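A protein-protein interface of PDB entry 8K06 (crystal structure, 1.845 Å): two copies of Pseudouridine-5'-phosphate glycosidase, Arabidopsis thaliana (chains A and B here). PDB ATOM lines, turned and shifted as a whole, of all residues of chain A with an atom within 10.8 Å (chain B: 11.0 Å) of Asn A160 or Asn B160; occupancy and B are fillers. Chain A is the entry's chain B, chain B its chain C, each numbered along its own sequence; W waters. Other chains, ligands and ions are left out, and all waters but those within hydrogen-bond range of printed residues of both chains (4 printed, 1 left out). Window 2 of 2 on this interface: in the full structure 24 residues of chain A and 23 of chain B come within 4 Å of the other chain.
The side-chain amide nitrogen (ND2) of Asn A160 is in hydrogen-bond range of the backbone carbonyl oxygen (O) of Asn B160.
OD1 of Asp B164 sits close to OE1 of Glu A195 (3.3 Å).
The backbone NH of Asp A189 is in hydrogen-bond range of the backbone carbonyl oxygen of Val A155 (2.8 Å).
The side-chain hydroxyl of Thr A193 is in hydrogen-bond range of the backbone NH of Val A155.
The side-chain carboxylate (OD2) of Asp A189 lies within salt-bridge range of the side-chain amino group (NZ) of Lys A192 (2.8 Å).
The backbone NH (N) of His B156 is in hydrogen-bond range of the backbone carbonyl oxygen (O) of Asp B164, 3.1 Å away.
O of His B158 is in hydrogen-bond range of OG of Ser B162 (3.5 Å).
The backbone NH (N) of Asp B164 is in hydrogen-bond range of the side-chain hydroxyl (OG) of Ser B162, at 3.0 Å.
SD of Met B163 touches CG1 of Val A155, at 3.9 Å.
CD1 of Ile A165 touches CE of Met B163 (3.8 Å).
Lys A192 touches His B161 (NZ to O, 3.5 Å).
O of Ser B162 touches CG of Lys A192, at 3.95 Å.
Glu A195 touches Ser B162 (CG to O, 3.2 Å).
Glu A195 touches Met B163.
Tyr A196 touches Met B163.
Asn B160 touches just one residue of chain A: Asn A160.
No residue of chain B comes within 4 Å of Ala A159.
No residue of chain B comes within 4 Å of His A161.
No residue of chain B comes within 4 Å of Ser A162.
No residue of chain A comes within 4 Å of Ala B159.
Of chain A, only Lys A192 (3.95 Å) and Glu A195 (3.2 Å) come within 4 Å of Ser B162.
Of the printed residues of chain B, Val A155 touches Met B163.
Of the printed residues of chain A, Asp B164 touches Glu A195 (3.3 Å).
His B158 touches none of the printed residues of chain A.
The nearest residue of chain B that does not touch Asn A160 is His B161 (4.5 Å).
The nearest printed residue of chain A that does not touch Asp B164 is Tyr A196 (6.5 Å).
Of the 18 printed residues of chain B, 5 touch a printed residue of chain A.
Hydrophobic or aromatic side chains of chain B that line the printed part of chain A: Met B163.
Val A155 touches Met B163, but with the chains exchanged Met A163 does not touch Val B155 (11.6 Å).
Glu A195 touches Ser B162, but with the chains exchanged Ser A162 does not touch Glu B195 (16.7 Å).
Glu A195 touches Asp B164, but with the chains exchanged Asp A164 does not touch Glu B195 (17.6 Å).
Tyr A196 touches Met B163, but with the chains exchanged Met A163 does not touch Tyr B196 (8.3 Å).
Of the 9 pairs that touch across the chains among the printed residues, 1 has its exchanged pair printed and touching as well.
Water W2 lies within hydrogen-bond range of OE2 of Glu A195 (2.4 Å) and OD2 of Asp B164 (3.2 Å).
Water W1 lies within hydrogen-bond range of O of Ser B162 (2.7 Å), N of Lys A192 (3.4 Å) and O of Pro A191 (3.4 Å).
Water W3 lies within hydrogen-bond range of OE1 of Glu A195 (2.8 Å), N of Ile B165 (3.2 Å) and O of Met B163 (3.5 Å).
Water W4 bridges O of His B161 (2.8 Å) and NZ of Lys A192 (3.2 Å).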
ATOM      1  N   GLY A 154      -8.520   1.319 -31.892  1.00  0.00           N
ATOM      2  CA  GLY A 154      -9.522   1.608 -30.878  1.00  0.00           C
ATOM      3  C   GLY A 154      -9.968   3.051 -30.896  1.00  0.00           C
ATOM      4  O   GLY A 154      -9.894   3.712 -31.936  1.00  0.00           O
ATOM      5  N   VAL A 155     -10.486   3.513 -29.758  1.00  0.00           N
ATOM      6  CA  VAL A 155     -10.843   4.919 -29.579  1.00  0.00           C
ATOM      7  C   VAL A 155      -9.575   5.694 -29.268  1.00  0.00           C
ATOM      8  O   VAL A 155      -8.851   5.361 -28.319  1.00  0.00           O
ATOM      9  CB  VAL A 155     -11.881   5.112 -28.447  1.00  0.00           C
ATOM     10  CG1 VAL A 155     -12.191   6.591 -28.285  1.00  0.00           C
ATOM     11  CG2 VAL A 155     -13.160   4.323 -28.757  1.00  0.00           C
ATOM     12  N   HIS A 156      -9.259   6.694 -30.099  1.00  0.00           N
ATOM     13  CA  HIS A 156      -8.020   7.441 -29.901  1.00  0.00           C
ATOM     14  C   HIS A 156      -8.156   8.385 -28.733  1.00  0.00           C
ATOM     15  O   HIS A 156      -9.266   8.721 -28.318  1.00  0.00           O
ATOM     16  CB  HIS A 156      -7.647   8.216 -31.167  1.00  0.00           C
ATOM     17  CG  HIS A 156      -7.196   7.335 -32.282  1.00  0.00           C
ATOM     18  ND1 HIS A 156      -5.886   7.279 -32.703  1.00  0.00           N
ATOM     19  CD2 HIS A 156      -7.871   6.432 -33.033  1.00  0.00           C
ATOM     20  CE1 HIS A 156      -5.778   6.397 -33.682  1.00  0.00           C
ATOM     21  NE2 HIS A 156      -6.970   5.867 -33.900  1.00  0.00           N
ATOM     22  N   ARG A 157      -7.024   8.777 -28.162  1.00  0.00           N
ATOM     23  CA  ARG A 157      -7.049   9.739 -27.080  1.00  0.00           C
ATOM     24  C   ARG A 157      -7.609  11.035 -27.637  1.00  0.00           C
ATOM     25  O   ARG A 157      -7.383  11.346 -28.797  1.00  0.00           O
ATOM     26  CB  ARG A 157      -5.650   9.933 -26.489  1.00  0.00           C
ATOM     27  CG  ARG A 157      -5.140   8.674 -25.837  1.00  0.00           C
ATOM     28  CD  ARG A 157      -3.729   8.826 -25.282  1.00  0.00           C
ATOM     29  NE  ARG A 157      -3.420   7.630 -24.509  1.00  0.00           N
ATOM     30  CZ  ARG A 157      -3.431   7.581 -23.182  1.00  0.00           C
ATOM     31  NH1 ARG A 157      -3.710   8.678 -22.481  1.00  0.00           N
ATOM     32  NH2 ARG A 157      -3.160   6.434 -22.558  1.00  0.00           N
ATOM     33  N   HIS A 158      -8.395  11.733 -26.820  1.00  0.00           N
ATOM     34  CA  HIS A 158      -9.026  13.001 -27.192  1.00  0.00           C
ATOM     35  C   HIS A 158     -10.099  12.825 -28.271  1.00  0.00           C
ATOM     36  O   HIS A 158     -10.377  13.751 -29.034  1.00  0.00           O
ATOM     37  CB  HIS A 158      -7.972  14.000 -27.680  1.00  0.00           C
ATOM     38  CG  HIS A 158      -6.839  14.198 -26.724  1.00  0.00           C
ATOM     39  ND1 HIS A 158      -7.030  14.385 -25.371  1.00  0.00           N
ATOM     40  CD2 HIS A 158      -5.501  14.246 -26.925  1.00  0.00           C
ATOM     41  CE1 HIS A 158      -5.857  14.531 -24.780  1.00  0.00           C
ATOM     42  NE2 HIS A 158      -4.914  14.457 -25.701  1.00  0.00           N
ATOM     43  N   ALA A 159     -10.694  11.638 -28.349  1.00  0.00           N
ATOM     44  CA  ALA A 159     -11.730  11.385 -29.361  1.00  0.00           C
ATOM     45  C   ALA A 159     -12.955  12.275 -29.141  1.00  0.00           C
ATOM     46  O   ALA A 159     -13.811  12.417 -30.029  1.00  0.00           O
ATOM     47  CB  ALA A 159     -12.139   9.902 -29.363  1.00  0.00           C
ATOM     48  N   ASN A 160     -13.050  12.871 -27.956  1.00  0.00           N
ATOM     49  CA  ASN A 160     -14.142  13.798 -27.683  1.00  0.00           C
ATOM     50  C   ASN A 160     -14.014  15.081 -28.495  1.00  0.00           C
ATOM     51  O   ASN A 160     -15.004  15.750 -28.757  1.00  0.00           O
ATOM     52  CB  ASN A 160     -14.210  14.110 -26.190  1.00  0.00           C
ATOM     53  CG  ASN A 160     -14.406  12.861 -25.360  1.00  0.00           C
ATOM     54  OD1 ASN A 160     -15.078  11.913 -25.799  1.00  0.00           O
ATOM     55  ND2 ASN A 160     -13.817  12.839 -24.156  1.00  0.00           N
ATOM     56  N   HIS A 161     -12.807  15.415 -28.930  1.00  0.00           N
ATOM     57  CA  HIS A 161     -12.659  16.553 -29.824  1.00  0.00           C
ATOM     58  C   HIS A 161     -12.486  16.120 -31.287  1.00  0.00           C
ATOM     59  O   HIS A 161     -12.648  16.928 -32.211  1.00  0.00           O
ATOM     60  CB  HIS A 161     -11.483  17.441 -29.427  1.00  0.00           C
ATOM     61  CG  HIS A 161     -11.319  18.626 -30.330  1.00  0.00           C
ATOM     62  ND1 HIS A 161     -12.396  19.342 -30.810  1.00  0.00           N
ATOM     63  CD2 HIS A 161     -10.218  19.178 -30.891  1.00  0.00           C
ATOM     64  CE1 HIS A 161     -11.962  20.309 -31.601  1.00  0.00           C
ATOM     65  NE2 HIS A 161     -10.646  20.230 -31.669  1.00  0.00           N
ATOM     66  N   SER A 162     -12.144  14.854 -31.505  1.00  0.00           N
ATOM     67  CA  SER A 162     -11.832  14.412 -32.859  1.00  0.00           C
ATOM     68  C   SER A 162     -12.819  13.409 -33.449  1.00  0.00           C
ATOM     69  O   SER A 162     -13.002  13.370 -34.675  1.00  0.00           O
ATOM     70  CB  SER A 162     -10.437  13.797 -32.890  1.00  0.00           C
ATOM     71  OG  SER A 162     -10.403  12.623 -32.104  1.00  0.00           O
ATOM     72  N   MET A 163     -13.438  12.602 -32.588  1.00  0.00           N
ATOM     73  CA  MET A 163     -14.200  11.440 -33.036  1.00  0.00           C
ATOM     74  C   MET A 163     -13.331  10.457 -33.808  1.00  0.00           C
ATOM     75  O   MET A 163     -13.839   9.693 -34.614  1.00  0.00           O
ATOM     76  CB  MET A 163     -15.416  11.854 -33.897  1.00  0.00           C
ATOM     77  CG  MET A 163     -16.462  12.613 -33.105  1.00  0.00           C
ATOM     78  SD  MET A 163     -18.110  12.555 -33.846  1.00  0.00           S
ATOM     79  CE  MET A 163     -18.680  10.944 -33.272  1.00  0.00           C
ATOM     80  N   ASP A 164     -12.023  10.461 -33.552  1.00  0.00           N
ATOM     81  CA  ASP A 164     -11.120   9.524 -34.215  1.00  0.00           C
ATOM     82  C   ASP A 164     -11.212   8.140 -33.567  1.00  0.00           C
ATOM     83  O   ASP A 164     -10.667   7.907 -32.488  1.00  0.00           O
ATOM     84  CB  ASP A 164      -9.685  10.064 -34.178  1.00  0.00           C
ATOM     85  CG  ASP A 164      -8.720   9.243 -35.023  1.00  0.00           C
ATOM     86  OD1 ASP A 164      -9.172   8.286 -35.680  1.00  0.00           O
ATOM     87  OD2 ASP A 164      -7.514   9.574 -35.050  1.00  0.00           O
ATOM     88  N   ILE A 165     -11.920   7.237 -34.237  1.00  0.00           N
ATOM     89  CA  ILE A 165     -12.206   5.897 -33.730  1.00  0.00           C
ATOM     90  C   ILE A 165     -12.005   4.861 -34.841  1.00  0.00           C
ATOM     91  O   ILE A 165     -12.552   4.995 -35.938  1.00  0.00           O
ATOM     92  CB  ILE A 165     -13.651   5.799 -33.205  1.00  0.00           C
ATOM     93  CG1 ILE A 165     -13.875   6.806 -32.060  1.00  0.00           C
ATOM     94  CG2 ILE A 165     -13.967   4.366 -32.754  1.00  0.00           C
ATOM     95  CD1 ILE A 165     -15.320   6.809 -31.521  1.00  0.00           C
ATOM     96  N   ASP A 189      -7.174   5.096 -26.105  1.00  0.00           N
ATOM     97  CA  ASP A 189      -7.946   5.257 -24.872  1.00  0.00           C
ATOM     98  C   ASP A 189      -8.578   3.928 -24.518  1.00  0.00           C
ATOM     99  O   ASP A 189      -9.596   3.551 -25.081  1.00  0.00           O
ATOM    100  CB  ASP A 189      -8.997   6.342 -25.055  1.00  0.00           C
ATOM    101  CG  ASP A 189      -9.678   6.748 -23.770  1.00  0.00           C
ATOM    102  OD1 ASP A 189     -10.048   5.879 -22.943  1.00  0.00           O
ATOM    103  OD2 ASP A 189      -9.854   7.976 -23.585  1.00  0.00           O
ATOM    104  N   PRO A 191     -10.148   2.501 -21.742  1.00  0.00           N
ATOM    105  CA  PRO A 191     -11.502   2.423 -21.187  1.00  0.00           C
ATOM    106  C   PRO A 191     -12.579   2.761 -22.219  1.00  0.00           C
ATOM    107  O   PRO A 191     -13.591   2.079 -22.281  1.00  0.00           O
ATOM    108  CB  PRO A 191     -11.481   3.465 -20.068  1.00  0.00           C
ATOM    109  CG  PRO A 191     -10.025   3.540 -19.666  1.00  0.00           C
ATOM    110  CD  PRO A 191      -9.265   3.362 -20.932  1.00  0.00           C
ATOM    111  N   LYS A 192     -12.367   3.795 -23.023  1.00  0.00           N
ATOM    112  CA  LYS A 192     -13.374   4.160 -24.003  1.00  0.00           C
ATOM    113  C   LYS A 192     -13.458   3.099 -25.094  1.00  0.00           C
ATOM    114  O   LYS A 192     -14.532   2.847 -25.636  1.00  0.00           O
ATOM    115  CB  LYS A 192     -13.062   5.524 -24.622  1.00  0.00           C
ATOM    116  CG  LYS A 192     -13.283   6.697 -23.678  1.00  0.00           C
ATOM    117  CD  LYS A 192     -13.073   8.025 -24.426  1.00  0.00           C
ATOM    118  CE  LYS A 192     -13.148   9.231 -23.471  1.00  0.00           C
ATOM    119  NZ  LYS A 192     -12.141   9.110 -22.393  1.00  0.00           N
ATOM    120  N   THR A 193     -12.331   2.490 -25.436  1.00  0.00           N
ATOM    121  CA  THR A 193     -12.364   1.427 -26.444  1.00  0.00           C
ATOM    122  C   THR A 193     -13.194   0.245 -25.916  1.00  0.00           C
ATOM    123  O   THR A 193     -13.971  -0.347 -26.652  1.00  0.00           O
ATOM    124  CB  THR A 193     -10.953   0.946 -26.812  1.00  0.00           C
ATOM    125  OG1 THR A 193     -10.212   2.029 -27.382  1.00  0.00           O
ATOM    126  CG2 THR A 193     -11.017  -0.204 -27.837  1.00  0.00           C
ATOM    127  N   GLU A 195     -15.667   0.387 -23.718  1.00  0.00           N
ATOM    128  CA  GLU A 195     -17.066   0.820 -23.749  1.00  0.00           C
ATOM    129  C   GLU A 195     -17.631   0.740 -25.181  1.00  0.00           C
ATOM    130  O   GLU A 195     -18.742   0.263 -25.386  1.00  0.00           O
ATOM    131  CB  GLU A 195     -17.220   2.252 -23.219  1.00  0.00           C
ATOM    132  CG  GLU A 195     -16.905   2.444 -21.741  1.00  0.00           C
ATOM    133  CD  GLU A 195     -17.923   1.798 -20.784  1.00  0.00           C
ATOM    134  OE1 GLU A 195     -19.001   1.341 -21.219  1.00  0.00           O
ATOM    135  OE2 GLU A 195     -17.628   1.742 -19.569  1.00  0.00           O
ATOM    136  N   TYR A 196     -16.853   1.186 -26.161  1.00  0.00           N
ATOM    137  CA  TYR A 196     -17.315   1.197 -27.549  1.00  0.00           C
ATOM    138  C   TYR A 196     -17.562  -0.239 -28.025  1.00  0.00           C
ATOM    139  O   TYR A 196     -18.566  -0.501 -28.662  1.00  0.00           O
ATOM    140  CB  TYR A 196     -16.298   1.899 -28.443  1.00  0.00           C
ATOM    141  CG  TYR A 196     -16.850   2.343 -29.777  1.00  0.00           C
ATOM    142  CD1 TYR A 196     -16.870   1.478 -30.869  1.00  0.00           C
ATOM    143  CD2 TYR A 196     -17.325   3.637 -29.953  1.00  0.00           C
ATOM    144  CE1 TYR A 196     -17.374   1.894 -32.090  1.00  0.00           C
ATOM    145  CE2 TYR A 196     -17.813   4.062 -31.178  1.00  0.00           C
ATOM    146  CZ  TYR A 196     -17.831   3.182 -32.235  1.00  0.00           C
ATOM    147  OH  TYR A 196     -18.303   3.603 -33.458  1.00  0.00           O
ATOM    148  N   GLY B 154     -29.686   3.146 -22.391  1.00  0.00           N
ATOM    149  CA  GLY B 154     -29.470   4.340 -23.190  1.00  0.00           C
ATOM    150  C   GLY B 154     -28.066   4.893 -23.073  1.00  0.00           C
ATOM    151  O   GLY B 154     -27.115   4.192 -22.737  1.00  0.00           O
ATOM    152  N   VAL B 155     -27.947   6.174 -23.377  1.00  0.00           N
ATOM    153  CA  VAL B 155     -26.702   6.895 -23.193  1.00  0.00           C
ATOM    154  C   VAL B 155     -26.606   7.285 -21.733  1.00  0.00           C
ATOM    155  O   VAL B 155     -27.494   7.955 -21.221  1.00  0.00           O
ATOM    156  CB  VAL B 155     -26.647   8.146 -24.067  1.00  0.00           C
ATOM    157  CG1 VAL B 155     -25.363   8.915 -23.781  1.00  0.00           C
ATOM    158  CG2 VAL B 155     -26.765   7.764 -25.538  1.00  0.00           C
ATOM    159  N   HIS B 156     -25.550   6.850 -21.061  1.00  0.00           N
ATOM    160  CA  HIS B 156     -25.408   7.144 -19.642  1.00  0.00           C
ATOM    161  C   HIS B 156     -24.990   8.598 -19.466  1.00  0.00           C
ATOM    162  O   HIS B 156     -24.449   9.219 -20.376  1.00  0.00           O
ATOM    163  CB  HIS B 156     -24.412   6.189 -18.981  1.00  0.00           C
ATOM    164  CG  HIS B 156     -24.923   4.784 -18.867  1.00  0.00           C
ATOM    165  ND1 HIS B 156     -25.304   4.222 -17.667  1.00  0.00           N
ATOM    166  CD2 HIS B 156     -25.162   3.844 -19.814  1.00  0.00           C
ATOM    167  CE1 HIS B 156     -25.737   2.990 -17.879  1.00  0.00           C
ATOM    168  NE2 HIS B 156     -25.647   2.731 -19.172  1.00  0.00           N
ATOM    169  N   ARG B 157     -25.252   9.159 -18.293  1.00  0.00           N
ATOM    170  CA  ARG B 157     -24.833  10.535 -18.073  1.00  0.00           C
ATOM    171  C   ARG B 157     -23.306  10.636 -18.166  1.00  0.00           C
ATOM    172  O   ARG B 157     -22.593   9.732 -17.736  1.00  0.00           O
ATOM    173  CB  ARG B 157     -25.336  11.029 -16.731  1.00  0.00           C
ATOM    174  CG  ARG B 157     -26.845  11.120 -16.679  1.00  0.00           C
ATOM    175  CD  ARG B 157     -27.279  11.556 -15.296  1.00  0.00           C
ATOM    176  NE  ARG B 157     -28.707  11.834 -15.197  1.00  0.00           N
ATOM    177  CZ  ARG B 157     -29.242  13.046 -15.096  1.00  0.00           C
ATOM    178  NH1 ARG B 157     -28.472  14.121 -15.070  1.00  0.00           N
ATOM    179  NH2 ARG B 157     -30.559  13.174 -14.990  1.00  0.00           N
ATOM    180  N   HIS B 158     -22.822  11.717 -18.770  1.00  0.00           N
ATOM    181  CA  HIS B 158     -21.385  11.940 -18.956  1.00  0.00           C
ATOM    182  C   HIS B 158     -20.717  10.958 -19.933  1.00  0.00           C
ATOM    183  O   HIS B 158     -19.518  10.710 -19.835  1.00  0.00           O
ATOM    184  CB  HIS B 158     -20.661  11.892 -17.604  1.00  0.00           C
ATOM    185  CG  HIS B 158     -21.208  12.853 -16.592  1.00  0.00           C
ATOM    186  ND1 HIS B 158     -21.484  14.171 -16.889  1.00  0.00           N
ATOM    187  CD2 HIS B 158     -21.507  12.694 -15.278  1.00  0.00           C
ATOM    188  CE1 HIS B 158     -21.944  14.779 -15.808  1.00  0.00           C
ATOM    189  NE2 HIS B 158     -21.967  13.904 -14.817  1.00  0.00           N
ATOM    190  N   ALA B 159     -21.477  10.425 -20.889  1.00  0.00           N
ATOM    191  CA  ALA B 159     -20.914   9.474 -21.862  1.00  0.00           C
ATOM    192  C   ALA B 159     -19.807  10.062 -22.760  1.00  0.00           C
ATOM    193  O   ALA B 159     -19.050   9.324 -23.387  1.00  0.00           O
ATOM    194  CB  ALA B 159     -22.030   8.900 -22.726  1.00  0.00           C
ATOM    195  N   ASN B 160     -19.720  11.383 -22.838  1.00  0.00           N
ATOM    196  CA  ASN B 160     -18.615  12.021 -23.554  1.00  0.00           C
ATOM    197  C   ASN B 160     -17.308  11.845 -22.809  1.00  0.00           C
ATOM    198  O   ASN B 160     -16.235  12.013 -23.369  1.00  0.00           O
ATOM    199  CB  ASN B 160     -18.915  13.485 -23.807  1.00  0.00           C
ATOM    200  CG  ASN B 160     -20.131  13.659 -24.676  1.00  0.00           C
ATOM    201  OD1 ASN B 160     -20.363  12.868 -25.600  1.00  0.00           O
ATOM    202  ND2 ASN B 160     -20.941  14.669 -24.371  1.00  0.00           N
ATOM    203  N   HIS B 161     -17.411  11.519 -21.530  1.00  0.00           N
ATOM    204  CA  HIS B 161     -16.242  11.212 -20.733  1.00  0.00           C
ATOM    205  C   HIS B 161     -16.057   9.701 -20.636  1.00  0.00           C
ATOM    206  O   HIS B 161     -14.968   9.219 -20.290  1.00  0.00           O
ATOM    207  CB  HIS B 161     -16.382  11.822 -19.332  1.00  0.00           C
ATOM    208  CG  HIS B 161     -15.230  11.524 -18.418  1.00  0.00           C
ATOM    209  ND1 HIS B 161     -15.402  11.184 -17.090  1.00  0.00           N
ATOM    210  CD2 HIS B 161     -13.892  11.508 -18.637  1.00  0.00           C
ATOM    211  CE1 HIS B 161     -14.223  10.975 -16.532  1.00  0.00           C
ATOM    212  NE2 HIS B 161     -13.289  11.166 -17.449  1.00  0.00           N
ATOM    213  N   SER B 162     -17.119   8.943 -20.905  1.00  0.00           N
ATOM    214  CA  SER B 162     -17.019   7.496 -20.737  1.00  0.00           C
ATOM    215  C   SER B 162     -17.263   6.683 -22.002  1.00  0.00           C
ATOM    216  O   SER B 162     -16.739   5.574 -22.123  1.00  0.00           O
ATOM    217  CB  SER B 162     -17.993   7.024 -19.667  1.00  0.00           C
ATOM    218  OG  SER B 162     -19.298   7.255 -20.119  1.00  0.00           O
ATOM    219  N   MET B 163     -18.087   7.226 -22.902  1.00  0.00           N
ATOM    220  CA  MET B 163     -18.662   6.491 -24.039  1.00  0.00           C
ATOM    221  C   MET B 163     -19.515   5.293 -23.589  1.00  0.00           C
ATOM    222  O   MET B 163     -19.717   4.351 -24.348  1.00  0.00           O
ATOM    223  CB  MET B 163     -17.563   6.022 -24.990  1.00  0.00           C
ATOM    224  CG  MET B 163     -16.833   7.175 -25.642  1.00  0.00           C
ATOM    225  SD  MET B 163     -15.960   6.705 -27.144  1.00  0.00           S
ATOM    226  CE  MET B 163     -17.314   6.707 -28.321  1.00  0.00           C
ATOM    227  N   ASP B 164     -20.017   5.345 -22.360  1.00  0.00           N
ATOM    228  CA  ASP B 164     -20.895   4.288 -21.824  1.00  0.00           C
ATOM    229  C   ASP B 164     -22.309   4.430 -22.404  1.00  0.00           C
ATOM    230  O   ASP B 164     -23.078   5.289 -21.994  1.00  0.00           O
ATOM    231  CB  ASP B 164     -20.916   4.368 -20.300  1.00  0.00           C
ATOM    232  CG  ASP B 164     -21.641   3.207 -19.643  1.00  0.00           C
ATOM    233  OD1 ASP B 164     -22.092   2.289 -20.350  1.00  0.00           O
ATOM    234  OD2 ASP B 164     -21.737   3.216 -18.399  1.00  0.00           O
ATOM    235  N   ILE B 165     -22.630   3.568 -23.369  1.00  0.00           N
ATOM    236  CA  ILE B 165     -23.879   3.614 -24.115  1.00  0.00           C
ATOM    237  C   ILE B 165     -24.411   2.198 -24.249  1.00  0.00           C
ATOM    238  O   ILE B 165     -23.664   1.289 -24.610  1.00  0.00           O
ATOM    239  CB  ILE B 165     -23.674   4.237 -25.519  1.00  0.00           C
ATOM    240  CG1 ILE B 165     -23.096   5.667 -25.398  1.00  0.00           C
ATOM    241  CG2 ILE B 165     -24.989   4.201 -26.297  1.00  0.00           C
ATOM    242  CD1 ILE B 165     -22.813   6.357 -26.753  1.00  0.00           C
ATOM    243  N   ASP B 189     -29.119   9.705 -19.866  1.00  0.00           N
ATOM    244  CA  ASP B 189     -29.223  11.001 -20.530  1.00  0.00           C
ATOM    245  C   ASP B 189     -30.292  10.920 -21.623  1.00  0.00           C
ATOM    246  O   ASP B 189     -30.037  10.398 -22.704  1.00  0.00           O
ATOM    247  CB  ASP B 189     -27.848  11.401 -21.111  1.00  0.00           C
ATOM    248  CG  ASP B 189     -27.802  12.838 -21.602  1.00  0.00           C
ATOM    249  OD1 ASP B 189     -28.767  13.291 -22.261  1.00  0.00           O
ATOM    250  OD2 ASP B 189     -26.776  13.509 -21.343  1.00  0.00           O
ATOM    251  N   PRO B 191     -32.091  13.225 -23.579  1.00  0.00           N
ATOM    252  CA  PRO B 191     -31.872  13.925 -24.856  1.00  0.00           C
ATOM    253  C   PRO B 191     -30.806  13.235 -25.739  1.00  0.00           C
ATOM    254  O   PRO B 191     -31.040  13.069 -26.948  1.00  0.00           O
ATOM    255  CB  PRO B 191     -31.418  15.320 -24.409  1.00  0.00           C
ATOM    256  CG  PRO B 191     -32.076  15.507 -23.065  1.00  0.00           C
ATOM    257  CD  PRO B 191     -32.042  14.142 -22.419  1.00  0.00           C
ATOM    258  N   LYS B 192     -29.695  12.797 -25.150  1.00  0.00           N
ATOM    259  CA  LYS B 192     -28.650  12.117 -25.938  1.00  0.00           C
ATOM    260  C   LYS B 192     -29.105  10.732 -26.398  1.00  0.00           C
ATOM    261  O   LYS B 192     -28.732  10.263 -27.468  1.00  0.00           O
ATOM    262  CB  LYS B 192     -27.341  11.973 -25.133  1.00  0.00           C
ATOM    263  CG  LYS B 192     -26.562  13.272 -24.958  1.00  0.00           C
ATOM    264  CD  LYS B 192     -25.243  13.006 -24.200  1.00  0.00           C
ATOM    265  CE  LYS B 192     -24.474  14.292 -23.919  1.00  0.00           C
ATOM    266  NZ  LYS B 192     -25.284  15.273 -23.155  1.00  0.00           N
ATOM    267  N   THR B 193     -29.893  10.061 -25.572  1.00  0.00           N
ATOM    268  CA  THR B 193     -30.404   8.747 -25.972  1.00  0.00           C
ATOM    269  C   THR B 193     -31.331   8.910 -27.183  1.00  0.00           C
ATOM    270  O   THR B 193     -31.257   8.120 -28.140  1.00  0.00           O
ATOM    271  CB  THR B 193     -31.134   8.043 -24.818  1.00  0.00           C
ATOM    272  OG1 THR B 193     -30.216   7.838 -23.723  1.00  0.00           O
ATOM    273  CG2 THR B 193     -31.689   6.706 -25.285  1.00  0.00           C
ATOM    274  N   GLU B 195     -31.174  11.329 -29.453  1.00  0.00           N
ATOM    275  CA  GLU B 195     -30.308  11.623 -30.605  1.00  0.00           C
ATOM    276  C   GLU B 195     -29.658  10.347 -31.137  1.00  0.00           C
ATOM    277  O   GLU B 195     -29.605  10.119 -32.351  1.00  0.00           O
ATOM    278  CB  GLU B 195     -29.218  12.636 -30.237  1.00  0.00           C
ATOM    279  CG  GLU B 195     -29.723  14.037 -29.909  1.00  0.00           C
ATOM    280  CD  GLU B 195     -30.209  14.824 -31.124  1.00  0.00           C
ATOM    281  OE1 GLU B 195     -29.958  14.405 -32.285  1.00  0.00           O
ATOM    282  OE2 GLU B 195     -30.880  15.864 -30.913  1.00  0.00           O
ATOM    283  N   TYR B 196     -29.176   9.511 -30.226  1.00  0.00           N
ATOM    284  CA  TYR B 196     -28.496   8.283 -30.631  1.00  0.00           C
ATOM    285  C   TYR B 196     -29.441   7.349 -31.390  1.00  0.00           C
ATOM    286  O   TYR B 196     -29.070   6.772 -32.430  1.00  0.00           O
ATOM    287  CB  TYR B 196     -27.923   7.586 -29.403  1.00  0.00           C
ATOM    288  CG  TYR B 196     -26.863   6.568 -29.710  1.00  0.00           C
ATOM    289  CD1 TYR B 196     -27.197   5.248 -29.992  1.00  0.00           C
ATOM    290  CD2 TYR B 196     -25.519   6.933 -29.745  1.00  0.00           C
ATOM    291  CE1 TYR B 196     -26.215   4.312 -30.278  1.00  0.00           C
ATOM    292  CE2 TYR B 196     -24.533   6.003 -30.018  1.00  0.00           C
ATOM    293  CZ  TYR B 196     -24.891   4.700 -30.290  1.00  0.00           C
ATOM    294  OH  TYR B 196     -23.898   3.784 -30.550  1.00  0.00           O
HETATM  295  O   HOH W   1     -14.504   5.002 -20.721  1.00  0.00           O
HETATM  296  O   HOH W   2     -19.000   1.861 -17.561  1.00  0.00           O
HETATM  297  O   HOH W   3     -20.581   1.105 -23.481  1.00  0.00           O
HETATM  298  O   HOH W   4     -13.035   7.145 -20.001  1.00  0.00           O
